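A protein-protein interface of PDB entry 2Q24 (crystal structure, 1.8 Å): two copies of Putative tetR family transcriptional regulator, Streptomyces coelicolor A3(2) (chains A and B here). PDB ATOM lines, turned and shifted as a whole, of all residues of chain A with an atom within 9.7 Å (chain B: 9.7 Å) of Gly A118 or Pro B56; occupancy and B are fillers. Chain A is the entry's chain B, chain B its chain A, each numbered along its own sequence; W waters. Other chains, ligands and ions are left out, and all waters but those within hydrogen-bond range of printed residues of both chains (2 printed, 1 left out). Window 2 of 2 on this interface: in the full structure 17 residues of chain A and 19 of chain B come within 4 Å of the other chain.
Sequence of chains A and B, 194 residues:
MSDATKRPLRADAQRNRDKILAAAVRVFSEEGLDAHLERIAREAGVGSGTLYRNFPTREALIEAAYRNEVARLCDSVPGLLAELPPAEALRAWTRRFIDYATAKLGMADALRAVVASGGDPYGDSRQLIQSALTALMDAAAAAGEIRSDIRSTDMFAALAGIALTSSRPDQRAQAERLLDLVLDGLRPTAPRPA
Glu B63 touches its own counterpart, Glu A63.
Positions printed for both chains: 59 and 63.
Of the 8 pairs that touch across the chains among the printed residues, 1 has its exchanged pair printed and touching as well.
Of the 21 printed residues of chain B, 5 touch a printed residue of chain A.
Printed residues of chain A that touch a printed residue of chain B: Glu A63, Gly A118, Asp A120 and Pro A121.
Among the printed residues, 8 pairs touch across the chains.
The side-chain hydroxyl (OG1) of Thr B57 is in hydrogen-bond range of the backbone NH (N) of Ala B60 (2.9 Å).
The side-chain carboxylate (OE2) of Glu B63 lies within salt-bridge range of the guanidinium group (NH1) of Arg B67, at 3.1 Å.
The side-chain carboxylate (OE2) of Glu A63 lies close to the side-chain carboxylate (OE2) of Glu B63.
The side-chain carboxylate (OE2) of Glu A63 lies within salt-bridge range of the guanidinium group (NH1) of Arg B67.
The backbone carbonyl oxygen (O) of Asp A120 lies within hydrogen-bond range of the guanidinium group (NH1) of Arg B67.
O of Pro A121 sits at hydrogen-bond distance from NH2 of Arg B67 (2.9 Å).
Of the printed residues of chain B, Glu A63 touches Glu B63 (2.6 Å) and Arg B67 (3.5 Å).
Ser A117 touches none of the printed residues of chain B.
No residue of chain B comes within 4 Å of Gly A119.
Of the printed residues of chain B, Asp A120 touches Glu B63 and Arg B67.
Printed residues of chain B within 4 Å of Pro A121: Arg B67.
Leu B51 touches none of the printed residues of chain A.
Pro B56 touches just one residue of chain A: Gly A118.
Of chain A, only Gly A118 (3.8 Å) comes within 4 Å of Thr B57.
Of the printed residues of chain A, Ala B60 touches Gly A118.
Of the printed residues of chain A, Glu B63 touches Glu A63 (2.6 Å) and Asp A120 (3.8 Å).
The nearest residue of chain B that does not touch Gly A118 is Phe B55 (6.3 Å).
The nearest residue of chain A that does not touch Pro B56 is Gly A119 (5.4 Å).
Gly A118 touches Pro B56.
Gly A118 touches Thr B57.
Gly A118 touches Ala B60.
Asp A120 touches Glu B63.
Water W2 bridges the side-chain hydroxyl (OG1) of Thr B57 (2.7 Å) and the backbone carbonyl oxygen (O) of Gly A118 (2.9 Å).
Water W1 lies within hydrogen-bond range of N of Asp A120, OE2 of Glu B63 and OE1 of Glu A63.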
ATOM      1  N   GLU A  59      15.540   7.752   5.598  1.00  0.00           N
ATOM      2  CA  GLU A  59      15.917   6.419   5.111  1.00  0.00           C
ATOM      3  C   GLU A  59      16.498   6.421   3.689  1.00  0.00           C
ATOM      4  O   GLU A  59      17.344   5.582   3.359  1.00  0.00           O
ATOM      5  CB  GLU A  59      14.828   5.344   5.300  1.00  0.00           C
ATOM      6  CG  GLU A  59      13.412   5.746   5.524  1.00  0.00           C
ATOM      7  CD  GLU A  59      13.188   6.671   6.712  1.00  0.00           C
ATOM      8  OE1 GLU A  59      13.282   6.244   7.885  1.00  0.00           O
ATOM      9  OE2 GLU A  59      12.894   7.841   6.446  1.00  0.00           O
ATOM     10  N   GLU A  63      20.169   4.880   3.014  1.00  0.00           N
ATOM     11  CA  GLU A  63      20.391   3.901   1.913  1.00  0.00           C
ATOM     12  C   GLU A  63      21.421   4.376   0.900  1.00  0.00           C
ATOM     13  O   GLU A  63      22.367   3.640   0.558  1.00  0.00           O
ATOM     14  CB  GLU A  63      19.076   3.551   1.197  1.00  0.00           C
ATOM     15  CG  GLU A  63      19.364   2.689  -0.018  1.00  0.00           C
ATOM     16  CD  GLU A  63      18.159   2.156  -0.707  1.00  0.00           C
ATOM     17  OE1 GLU A  63      17.081   2.084  -0.091  1.00  0.00           O
ATOM     18  OE2 GLU A  63      18.310   1.838  -1.909  1.00  0.00           O
ATOM     19  N   LEU A 111      20.525   1.407   9.371  1.00  0.00           N
ATOM     20  CA  LEU A 111      20.241   0.414   8.337  1.00  0.00           C
ATOM     21  C   LEU A 111      18.964  -0.379   8.650  1.00  0.00           C
ATOM     22  O   LEU A 111      18.155  -0.634   7.769  1.00  0.00           O
ATOM     23  CB  LEU A 111      21.444  -0.511   8.127  1.00  0.00           C
ATOM     24  CG  LEU A 111      22.670   0.181   7.490  1.00  0.00           C
ATOM     25  CD1 LEU A 111      23.967  -0.676   7.668  1.00  0.00           C
ATOM     26  CD2 LEU A 111      22.470   0.556   5.980  1.00  0.00           C
ATOM     27  N   ARG A 112      18.797  -0.752   9.913  1.00  0.00           N
ATOM     28  CA  ARG A 112      17.540  -1.360  10.413  1.00  0.00           C
ATOM     29  C   ARG A 112      16.294  -0.533  10.068  1.00  0.00           C
ATOM     30  O   ARG A 112      15.264  -1.090   9.684  1.00  0.00           O
ATOM     31  CB  ARG A 112      17.610  -1.489  11.922  1.00  0.00           C
ATOM     32  CG  ARG A 112      17.164  -2.837  12.478  1.00  0.00           C
ATOM     33  CD  ARG A 112      18.378  -3.797  12.544  1.00  0.00           C
ATOM     34  NE  ARG A 112      19.456  -3.389  13.472  1.00  0.00           N
ATOM     35  CZ  ARG A 112      19.296  -2.724  14.626  1.00  0.00           C
ATOM     36  NH1 ARG A 112      18.087  -2.352  15.048  1.00  0.00           N
ATOM     37  NH2 ARG A 112      20.360  -2.423  15.366  1.00  0.00           N
ATOM     38  N   ALA A 113      16.398   0.789  10.198  1.00  0.00           N
ATOM     39  CA  ALA A 113      15.265   1.702   9.991  1.00  0.00           C
ATOM     40  C   ALA A 113      14.901   1.818   8.505  1.00  0.00           C
ATOM     41  O   ALA A 113      13.734   2.047   8.148  1.00  0.00           O
ATOM     42  CB  ALA A 113      15.578   3.064  10.570  1.00  0.00           C
ATOM     43  N   VAL A 114      15.894   1.641   7.638  1.00  0.00           N
ATOM     44  CA  VAL A 114      15.610   1.556   6.218  1.00  0.00           C
ATOM     45  C   VAL A 114      14.768   0.285   5.928  1.00  0.00           C
ATOM     46  O   VAL A 114      13.766   0.359   5.196  1.00  0.00           O
ATOM     47  CB  VAL A 114      16.895   1.531   5.368  1.00  0.00           C
ATOM     48  CG1 VAL A 114      16.555   1.399   3.897  1.00  0.00           C
ATOM     49  CG2 VAL A 114      17.717   2.791   5.601  1.00  0.00           C
ATOM     50  N   VAL A 115      15.178  -0.845   6.494  1.00  0.00           N
ATOM     51  CA  VAL A 115      14.419  -2.084   6.367  1.00  0.00           C
ATOM     52  C   VAL A 115      12.987  -1.908   6.859  1.00  0.00           C
ATOM     53  O   VAL A 115      12.033  -2.213   6.145  1.00  0.00           O
ATOM     54  CB  VAL A 115      15.083  -3.234   7.147  1.00  0.00           C
ATOM     55  CG1 VAL A 115      14.248  -4.500   7.038  1.00  0.00           C
ATOM     56  CG2 VAL A 115      16.496  -3.474   6.638  1.00  0.00           C
ATOM     57  N   ALA A 116      12.846  -1.413   8.084  1.00  0.00           N
ATOM     58  CA  ALA A 116      11.557  -1.413   8.767  1.00  0.00           C
ATOM     59  C   ALA A 116      10.567  -0.481   8.075  1.00  0.00           C
ATOM     60  O   ALA A 116       9.376  -0.482   8.390  1.00  0.00           O
ATOM     61  CB  ALA A 116      11.729  -1.021  10.226  1.00  0.00           C
ATOM     62  N   SER A 117      11.067   0.313   7.135  1.00  0.00           N
ATOM     63  CA  SER A 117      10.200   1.137   6.278  1.00  0.00           C
ATOM     64  C   SER A 117      10.011   0.498   4.898  1.00  0.00           C
ATOM     65  O   SER A 117       9.400   1.097   4.002  1.00  0.00           O
ATOM     66  CB  SER A 117      10.773   2.556   6.102  1.00  0.00           C
ATOM     67  OG  SER A 117      10.037   3.519   6.857  1.00  0.00           O
ATOM     68  N   GLY A 118      10.530  -0.718   4.739  1.00  0.00           N
ATOM     69  CA  GLY A 118      10.279  -1.526   3.545  1.00  0.00           C
ATOM     70  C   GLY A 118      11.322  -1.359   2.451  1.00  0.00           C
ATOM     71  O   GLY A 118      11.107  -1.805   1.325  1.00  0.00           O
ATOM     72  N   GLY A 119      12.437  -0.711   2.786  1.00  0.00           N
ATOM     73  CA  GLY A 119      13.517  -0.490   1.824  1.00  0.00           C
ATOM     74  C   GLY A 119      14.628  -1.510   2.011  1.00  0.00           C
ATOM     75  O   GLY A 119      14.605  -2.320   2.947  1.00  0.00           O
ATOM     76  N   ASP A 120      15.615  -1.486   1.120  1.00  0.00           N
ATOM     77  CA  ASP A 120      16.674  -2.513   1.174  1.00  0.00           C
ATOM     78  C   ASP A 120      17.987  -1.886   0.828  1.00  0.00           C
ATOM     79  O   ASP A 120      18.292  -1.694  -0.355  1.00  0.00           O
ATOM     80  CB  ASP A 120      16.379  -3.717   0.251  1.00  0.00           C
ATOM     81  CG  ASP A 120      17.626  -4.626   0.047  1.00  0.00           C
ATOM     82  OD1 ASP A 120      18.412  -4.825   1.008  1.00  0.00           O
ATOM     83  OD2 ASP A 120      17.813  -5.124  -1.075  1.00  0.00           O
ATOM     84  N   PRO A 121      18.769  -1.524   1.863  1.00  0.00           N
ATOM     85  CA  PRO A 121      20.023  -0.833   1.621  1.00  0.00           C
ATOM     86  C   PRO A 121      21.061  -1.734   0.936  1.00  0.00           C
ATOM     87  O   PRO A 121      21.940  -1.210   0.276  1.00  0.00           O
ATOM     88  CB  PRO A 121      20.513  -0.447   3.024  1.00  0.00           C
ATOM     89  CG  PRO A 121      19.719  -1.255   3.969  1.00  0.00           C
ATOM     90  CD  PRO A 121      18.498  -1.747   3.296  1.00  0.00           C
ATOM     91  N   ILE B  20      14.414 -15.095  -8.636  1.00  0.00           N
ATOM     92  CA  ILE B  20      13.335 -14.130  -8.380  1.00  0.00           C
ATOM     93  C   ILE B  20      13.612 -12.869  -9.196  1.00  0.00           C
ATOM     94  O   ILE B  20      12.729 -12.310  -9.840  1.00  0.00           O
ATOM     95  CB  ILE B  20      13.212 -13.777  -6.883  1.00  0.00           C
ATOM     96  CG1 ILE B  20      12.399 -14.831  -6.114  1.00  0.00           C
ATOM     97  CG2 ILE B  20      12.507 -12.441  -6.681  1.00  0.00           C
ATOM     98  CD1 ILE B  20      12.631 -14.743  -4.568  1.00  0.00           C
ATOM     99  N   LEU B  21      14.856 -12.391  -9.135  1.00  0.00           N
ATOM    100  CA  LEU B  21      15.153 -11.086  -9.757  1.00  0.00           C
ATOM    101  C   LEU B  21      15.205 -11.169 -11.285  1.00  0.00           C
ATOM    102  O   LEU B  21      14.784 -10.238 -11.952  1.00  0.00           O
ATOM    103  CB  LEU B  21      16.438 -10.491  -9.151  1.00  0.00           C
ATOM    104  CG  LEU B  21      16.271 -10.115  -7.662  1.00  0.00           C
ATOM    105  CD1 LEU B  21      17.651  -9.648  -7.088  1.00  0.00           C
ATOM    106  CD2 LEU B  21      15.159  -9.078  -7.336  1.00  0.00           C
ATOM    107  N   LEU B  37       2.650  -9.629  -8.987  1.00  0.00           N
ATOM    108  CA  LEU B  37       3.789 -10.182  -8.198  1.00  0.00           C
ATOM    109  C   LEU B  37       3.753 -11.711  -8.022  1.00  0.00           C
ATOM    110  O   LEU B  37       4.805 -12.363  -7.963  1.00  0.00           O
ATOM    111  CB  LEU B  37       3.879  -9.522  -6.830  1.00  0.00           C
ATOM    112  CG  LEU B  37       3.926  -7.997  -6.879  1.00  0.00           C
ATOM    113  CD1 LEU B  37       3.807  -7.437  -5.438  1.00  0.00           C
ATOM    114  CD2 LEU B  37       5.199  -7.501  -7.562  1.00  0.00           C
ATOM    115  N   SER B  48       4.581 -16.848  -2.459  1.00  0.00           N
ATOM    116  CA  SER B  48       4.488 -15.378  -2.383  1.00  0.00           C
ATOM    117  C   SER B  48       4.850 -14.815  -0.982  1.00  0.00           C
ATOM    118  O   SER B  48       5.206 -13.657  -0.869  1.00  0.00           O
ATOM    119  CB  SER B  48       3.149 -14.850  -2.889  1.00  0.00           C
ATOM    120  OG  SER B  48       2.145 -15.106  -1.941  1.00  0.00           O
ATOM    121  N   GLY B  49       4.766 -15.648   0.058  1.00  0.00           N
ATOM    122  CA  GLY B  49       5.291 -15.309   1.385  1.00  0.00           C
ATOM    123  C   GLY B  49       6.805 -15.135   1.307  1.00  0.00           C
ATOM    124  O   GLY B  49       7.371 -14.189   1.857  1.00  0.00           O
ATOM    125  N   THR B  50       7.462 -16.051   0.601  1.00  0.00           N
ATOM    126  CA  THR B  50       8.903 -15.966   0.394  1.00  0.00           C
ATOM    127  C   THR B  50       9.289 -14.711  -0.384  1.00  0.00           C
ATOM    128  O   THR B  50      10.258 -14.022  -0.020  1.00  0.00           O
ATOM    129  CB  THR B  50       9.427 -17.231  -0.296  1.00  0.00           C
ATOM    130  OG1 THR B  50       9.217 -18.331   0.582  1.00  0.00           O
ATOM    131  CG2 THR B  50      10.908 -17.142  -0.597  1.00  0.00           C
ATOM    132  N   LEU B  51       8.542 -14.418  -1.455  1.00  0.00           N
ATOM    133  CA  LEU B  51       8.822 -13.225  -2.264  1.00  0.00           C
ATOM    134  C   LEU B  51       8.738 -12.011  -1.353  1.00  0.00           C
ATOM    135  O   LEU B  51       9.677 -11.187  -1.289  1.00  0.00           O
ATOM    136  CB  LEU B  51       7.853 -13.080  -3.457  1.00  0.00           C
ATOM    137  CG  LEU B  51       8.101 -11.906  -4.449  1.00  0.00           C
ATOM    138  CD1 LEU B  51       9.568 -11.781  -4.832  1.00  0.00           C
ATOM    139  CD2 LEU B  51       7.240 -12.086  -5.711  1.00  0.00           C
ATOM    140  N   TYR B  52       7.630 -11.951  -0.611  1.00  0.00           N
ATOM    141  CA  TYR B  52       7.327 -10.823   0.288  1.00  0.00           C
ATOM    142  C   TYR B  52       8.346 -10.665   1.404  1.00  0.00           C
ATOM    143  O   TYR B  52       8.690  -9.544   1.760  1.00  0.00           O
ATOM    144  CB  TYR B  52       5.920 -10.968   0.886  1.00  0.00           C
ATOM    145  CG  TYR B  52       5.515  -9.847   1.827  1.00  0.00           C
ATOM    146  CD1 TYR B  52       5.226  -8.550   1.348  1.00  0.00           C
ATOM    147  CD2 TYR B  52       5.422 -10.072   3.205  1.00  0.00           C
ATOM    148  CE1 TYR B  52       4.856  -7.519   2.226  1.00  0.00           C
ATOM    149  CE2 TYR B  52       5.049  -9.060   4.084  1.00  0.00           C
ATOM    150  CZ  TYR B  52       4.782  -7.784   3.593  1.00  0.00           C
ATOM    151  OH  TYR B  52       4.400  -6.808   4.485  1.00  0.00           O
ATOM    152  N   ARG B  53       8.829 -11.769   1.972  1.00  0.00           N
ATOM    153  CA  ARG B  53       9.831 -11.652   3.046  1.00  0.00           C
ATOM    154  C   ARG B  53      11.124 -11.044   2.551  1.00  0.00           C
ATOM    155  O   ARG B  53      11.806 -10.324   3.291  1.00  0.00           O
ATOM    156  CB  ARG B  53      10.102 -13.002   3.727  1.00  0.00           C
ATOM    157  CG  ARG B  53       8.979 -13.411   4.689  1.00  0.00           C
ATOM    158  CD  ARG B  53       9.344 -14.652   5.541  1.00  0.00           C
ATOM    159  NE  ARG B  53      10.030 -15.686   4.752  1.00  0.00           N
ATOM    160  CZ  ARG B  53       9.448 -16.755   4.201  1.00  0.00           C
ATOM    161  NH1 ARG B  53       8.140 -16.980   4.342  1.00  0.00           N
ATOM    162  NH2 ARG B  53      10.189 -17.618   3.499  1.00  0.00           N
ATOM    163  N   ASN B  54      11.453 -11.314   1.292  1.00  0.00           N
ATOM    164  CA  ASN B  54      12.687 -10.794   0.709  1.00  0.00           C
ATOM    165  C   ASN B  54      12.566  -9.413   0.082  1.00  0.00           C
ATOM    166  O   ASN B  54      13.510  -8.601   0.151  1.00  0.00           O
ATOM    167  CB  ASN B  54      13.235 -11.796  -0.297  1.00  0.00           C
ATOM    168  CG  ASN B  54      13.614 -13.108   0.354  1.00  0.00           C
ATOM    169  OD1 ASN B  54      12.984 -14.128   0.127  1.00  0.00           O
ATOM    170  ND2 ASN B  54      14.610 -13.066   1.212  1.00  0.00           N
ATOM    171  N   PHE B  55      11.396  -9.133  -0.483  1.00  0.00           N
ATOM    172  CA  PHE B  55      11.140  -7.908  -1.255  1.00  0.00           C
ATOM    173  C   PHE B  55       9.715  -7.494  -0.903  1.00  0.00           C
ATOM    174  O   PHE B  55       8.780  -7.887  -1.588  1.00  0.00           O
ATOM    175  CB  PHE B  55      11.265  -8.199  -2.758  1.00  0.00           C
ATOM    176  CG  PHE B  55      12.623  -8.755  -3.139  1.00  0.00           C
ATOM    177  CD1 PHE B  55      13.739  -7.941  -3.092  1.00  0.00           C
ATOM    178  CD2 PHE B  55      12.783 -10.104  -3.475  1.00  0.00           C
ATOM    179  CE1 PHE B  55      15.024  -8.451  -3.393  1.00  0.00           C
ATOM    180  CE2 PHE B  55      14.051 -10.620  -3.771  1.00  0.00           C
ATOM    181  CZ  PHE B  55      15.169  -9.779  -3.731  1.00  0.00           C
ATOM    182  N   PRO B  56       9.561  -6.774   0.206  1.00  0.00           N
ATOM    183  CA  PRO B  56       8.230  -6.483   0.757  1.00  0.00           C
ATOM    184  C   PRO B  56       7.348  -5.522  -0.084  1.00  0.00           C
ATOM    185  O   PRO B  56       6.126  -5.510   0.068  1.00  0.00           O
ATOM    186  CB  PRO B  56       8.542  -5.892   2.134  1.00  0.00           C
ATOM    187  CG  PRO B  56       9.931  -5.397   2.071  1.00  0.00           C
ATOM    188  CD  PRO B  56      10.656  -6.200   1.015  1.00  0.00           C
ATOM    189  N   THR B  57       7.951  -4.717  -0.958  1.00  0.00           N
ATOM    190  CA  THR B  57       7.151  -3.780  -1.763  1.00  0.00           C
ATOM    191  C   THR B  57       7.525  -3.966  -3.226  1.00  0.00           C
ATOM    192  O   THR B  57       8.628  -4.434  -3.543  1.00  0.00           O
ATOM    193  CB  THR B  57       7.382  -2.303  -1.378  1.00  0.00           C
ATOM    194  OG1 THR B  57       8.735  -1.926  -1.679  1.00  0.00           O
ATOM    195  CG2 THR B  57       7.127  -2.061   0.104  1.00  0.00           C
ATOM    196  N   ARG B  58       6.621  -3.571  -4.113  1.00  0.00           N
ATOM    197  CA  ARG B  58       6.959  -3.679  -5.512  1.00  0.00           C
ATOM    198  C   ARG B  58       8.075  -2.742  -5.883  1.00  0.00           C
ATOM    199  O   ARG B  58       8.879  -3.101  -6.725  1.00  0.00           O
ATOM    200  CB  ARG B  58       5.721  -3.594  -6.435  1.00  0.00           C
ATOM    201  CG  ARG B  58       5.110  -2.278  -6.582  1.00  0.00           C
ATOM    202  CD  ARG B  58       3.930  -2.309  -7.629  1.00  0.00           C
ATOM    203  NE  ARG B  58       3.019  -3.397  -7.300  1.00  0.00           N
ATOM    204  CZ  ARG B  58       2.717  -4.421  -8.100  1.00  0.00           C
ATOM    205  NH1 ARG B  58       3.206  -4.504  -9.335  1.00  0.00           N
ATOM    206  NH2 ARG B  58       1.904  -5.342  -7.643  1.00  0.00           N
ATOM    207  N   GLU B  59       8.172  -1.577  -5.232  1.00  0.00           N
ATOM    208  CA  GLU B  59       9.305  -0.679  -5.528  1.00  0.00           C
ATOM    209  C   GLU B  59      10.612  -1.295  -5.081  1.00  0.00           C
ATOM    210  O   GLU B  59      11.617  -1.140  -5.783  1.00  0.00           O
ATOM    211  CB  GLU B  59       9.177   0.720  -4.892  1.00  0.00           C
ATOM    212  CG  GLU B  59       7.799   1.344  -4.993  1.00  0.00           C
ATOM    213  CD  GLU B  59       6.864   0.870  -3.868  1.00  0.00           C
ATOM    214  OE1 GLU B  59       6.092  -0.064  -4.138  1.00  0.00           O
ATOM    215  OE2 GLU B  59       6.900   1.418  -2.711  1.00  0.00           O
ATOM    216  N   ALA B  60      10.617  -1.975  -3.928  1.00  0.00           N
ATOM    217  CA  ALA B  60      11.871  -2.648  -3.508  1.00  0.00           C
ATOM    218  C   ALA B  60      12.286  -3.716  -4.511  1.00  0.00           C
ATOM    219  O   ALA B  60      13.466  -3.847  -4.820  1.00  0.00           O
ATOM    220  CB  ALA B  60      11.749  -3.276  -2.118  1.00  0.00           C
ATOM    221  N   LEU B  61      11.291  -4.474  -5.011  1.00  0.00           N
ATOM    222  CA  LEU B  61      11.555  -5.526  -5.986  1.00  0.00           C
ATOM    223  C   LEU B  61      12.122  -4.955  -7.296  1.00  0.00           C
ATOM    224  O   LEU B  61      13.059  -5.503  -7.857  1.00  0.00           O
ATOM    225  CB  LEU B  61      10.297  -6.344  -6.262  1.00  0.00           C
ATOM    226  CG  LEU B  61      10.454  -7.514  -7.237  1.00  0.00           C
ATOM    227  CD1 LEU B  61      11.420  -8.534  -6.642  1.00  0.00           C
ATOM    228  CD2 LEU B  61       9.050  -8.143  -7.356  1.00  0.00           C
ATOM    229  N   ILE B  62      11.521  -3.874  -7.784  1.00  0.00           N
ATOM    230  CA  ILE B  62      11.968  -3.216  -9.020  1.00  0.00           C
ATOM    231  C   ILE B  62      13.412  -2.762  -8.847  1.00  0.00           C
ATOM    232  O   ILE B  62      14.281  -3.027  -9.722  1.00  0.00           O
ATOM    233  CB  ILE B  62      11.107  -1.970  -9.332  1.00  0.00           C
ATOM    234  CG1 ILE B  62       9.736  -2.420  -9.809  1.00  0.00           C
ATOM    235  CG2 ILE B  62      11.719  -1.138 -10.473  1.00  0.00           C
ATOM    236  CD1 ILE B  62       8.637  -1.348  -9.646  1.00  0.00           C
ATOM    237  N   GLU B  63      13.645  -2.033  -7.749  1.00  0.00           N
ATOM    238  CA  GLU B  63      14.991  -1.512  -7.464  1.00  0.00           C
ATOM    239  C   GLU B  63      15.994  -2.673  -7.322  1.00  0.00           C
ATOM    240  O   GLU B  63      17.132  -2.593  -7.833  1.00  0.00           O
ATOM    241  CB  GLU B  63      14.995  -0.636  -6.214  1.00  0.00           C
ATOM    242  CG  GLU B  63      16.438  -0.352  -5.734  1.00  0.00           C
ATOM    243  CD  GLU B  63      16.553   0.580  -4.526  1.00  0.00           C
ATOM    244  OE1 GLU B  63      16.156   1.751  -4.628  1.00  0.00           O
ATOM    245  OE2 GLU B  63      17.079   0.130  -3.478  1.00  0.00           O
ATOM    246  N   ALA B  64      15.599  -3.757  -6.654  1.00  0.00           N
ATOM    247  CA  ALA B  64      16.530  -4.909  -6.463  1.00  0.00           C
ATOM    248  C   ALA B  64      16.869  -5.559  -7.787  1.00  0.00           C
ATOM    249  O   ALA B  64      18.009  -5.978  -8.025  1.00  0.00           O
ATOM    250  CB  ALA B  64      15.944  -5.928  -5.479  1.00  0.00           C
ATOM    251  N   ARG B  67      19.294  -3.283  -9.569  1.00  0.00           N
ATOM    252  CA  ARG B  67      20.605  -3.389  -8.919  1.00  0.00           C
ATOM    253  C   ARG B  67      21.284  -4.718  -9.238  1.00  0.00           C
ATOM    254  O   ARG B  67      22.502  -4.790  -9.412  1.00  0.00           O
ATOM    255  CB  ARG B  67      20.419  -3.248  -7.396  1.00  0.00           C
ATOM    256  CG  ARG B  67      20.119  -1.766  -7.071  1.00  0.00           C
ATOM    257  CD  ARG B  67      19.793  -1.526  -5.569  1.00  0.00           C
ATOM    258  NE  ARG B  67      20.945  -1.710  -4.660  1.00  0.00           N
ATOM    259  CZ  ARG B  67      20.902  -1.522  -3.339  1.00  0.00           C
ATOM    260  NH1 ARG B  67      19.751  -1.218  -2.728  1.00  0.00           N
ATOM    261  NH2 ARG B  67      22.003  -1.696  -2.607  1.00  0.00           N
HETATM  262  O   HOH W   1      15.176  -0.157  -1.240  1.00  0.00           O
HETATM  263  O   HOH W   2      10.085   0.114  -0.527  1.00  0.00           O
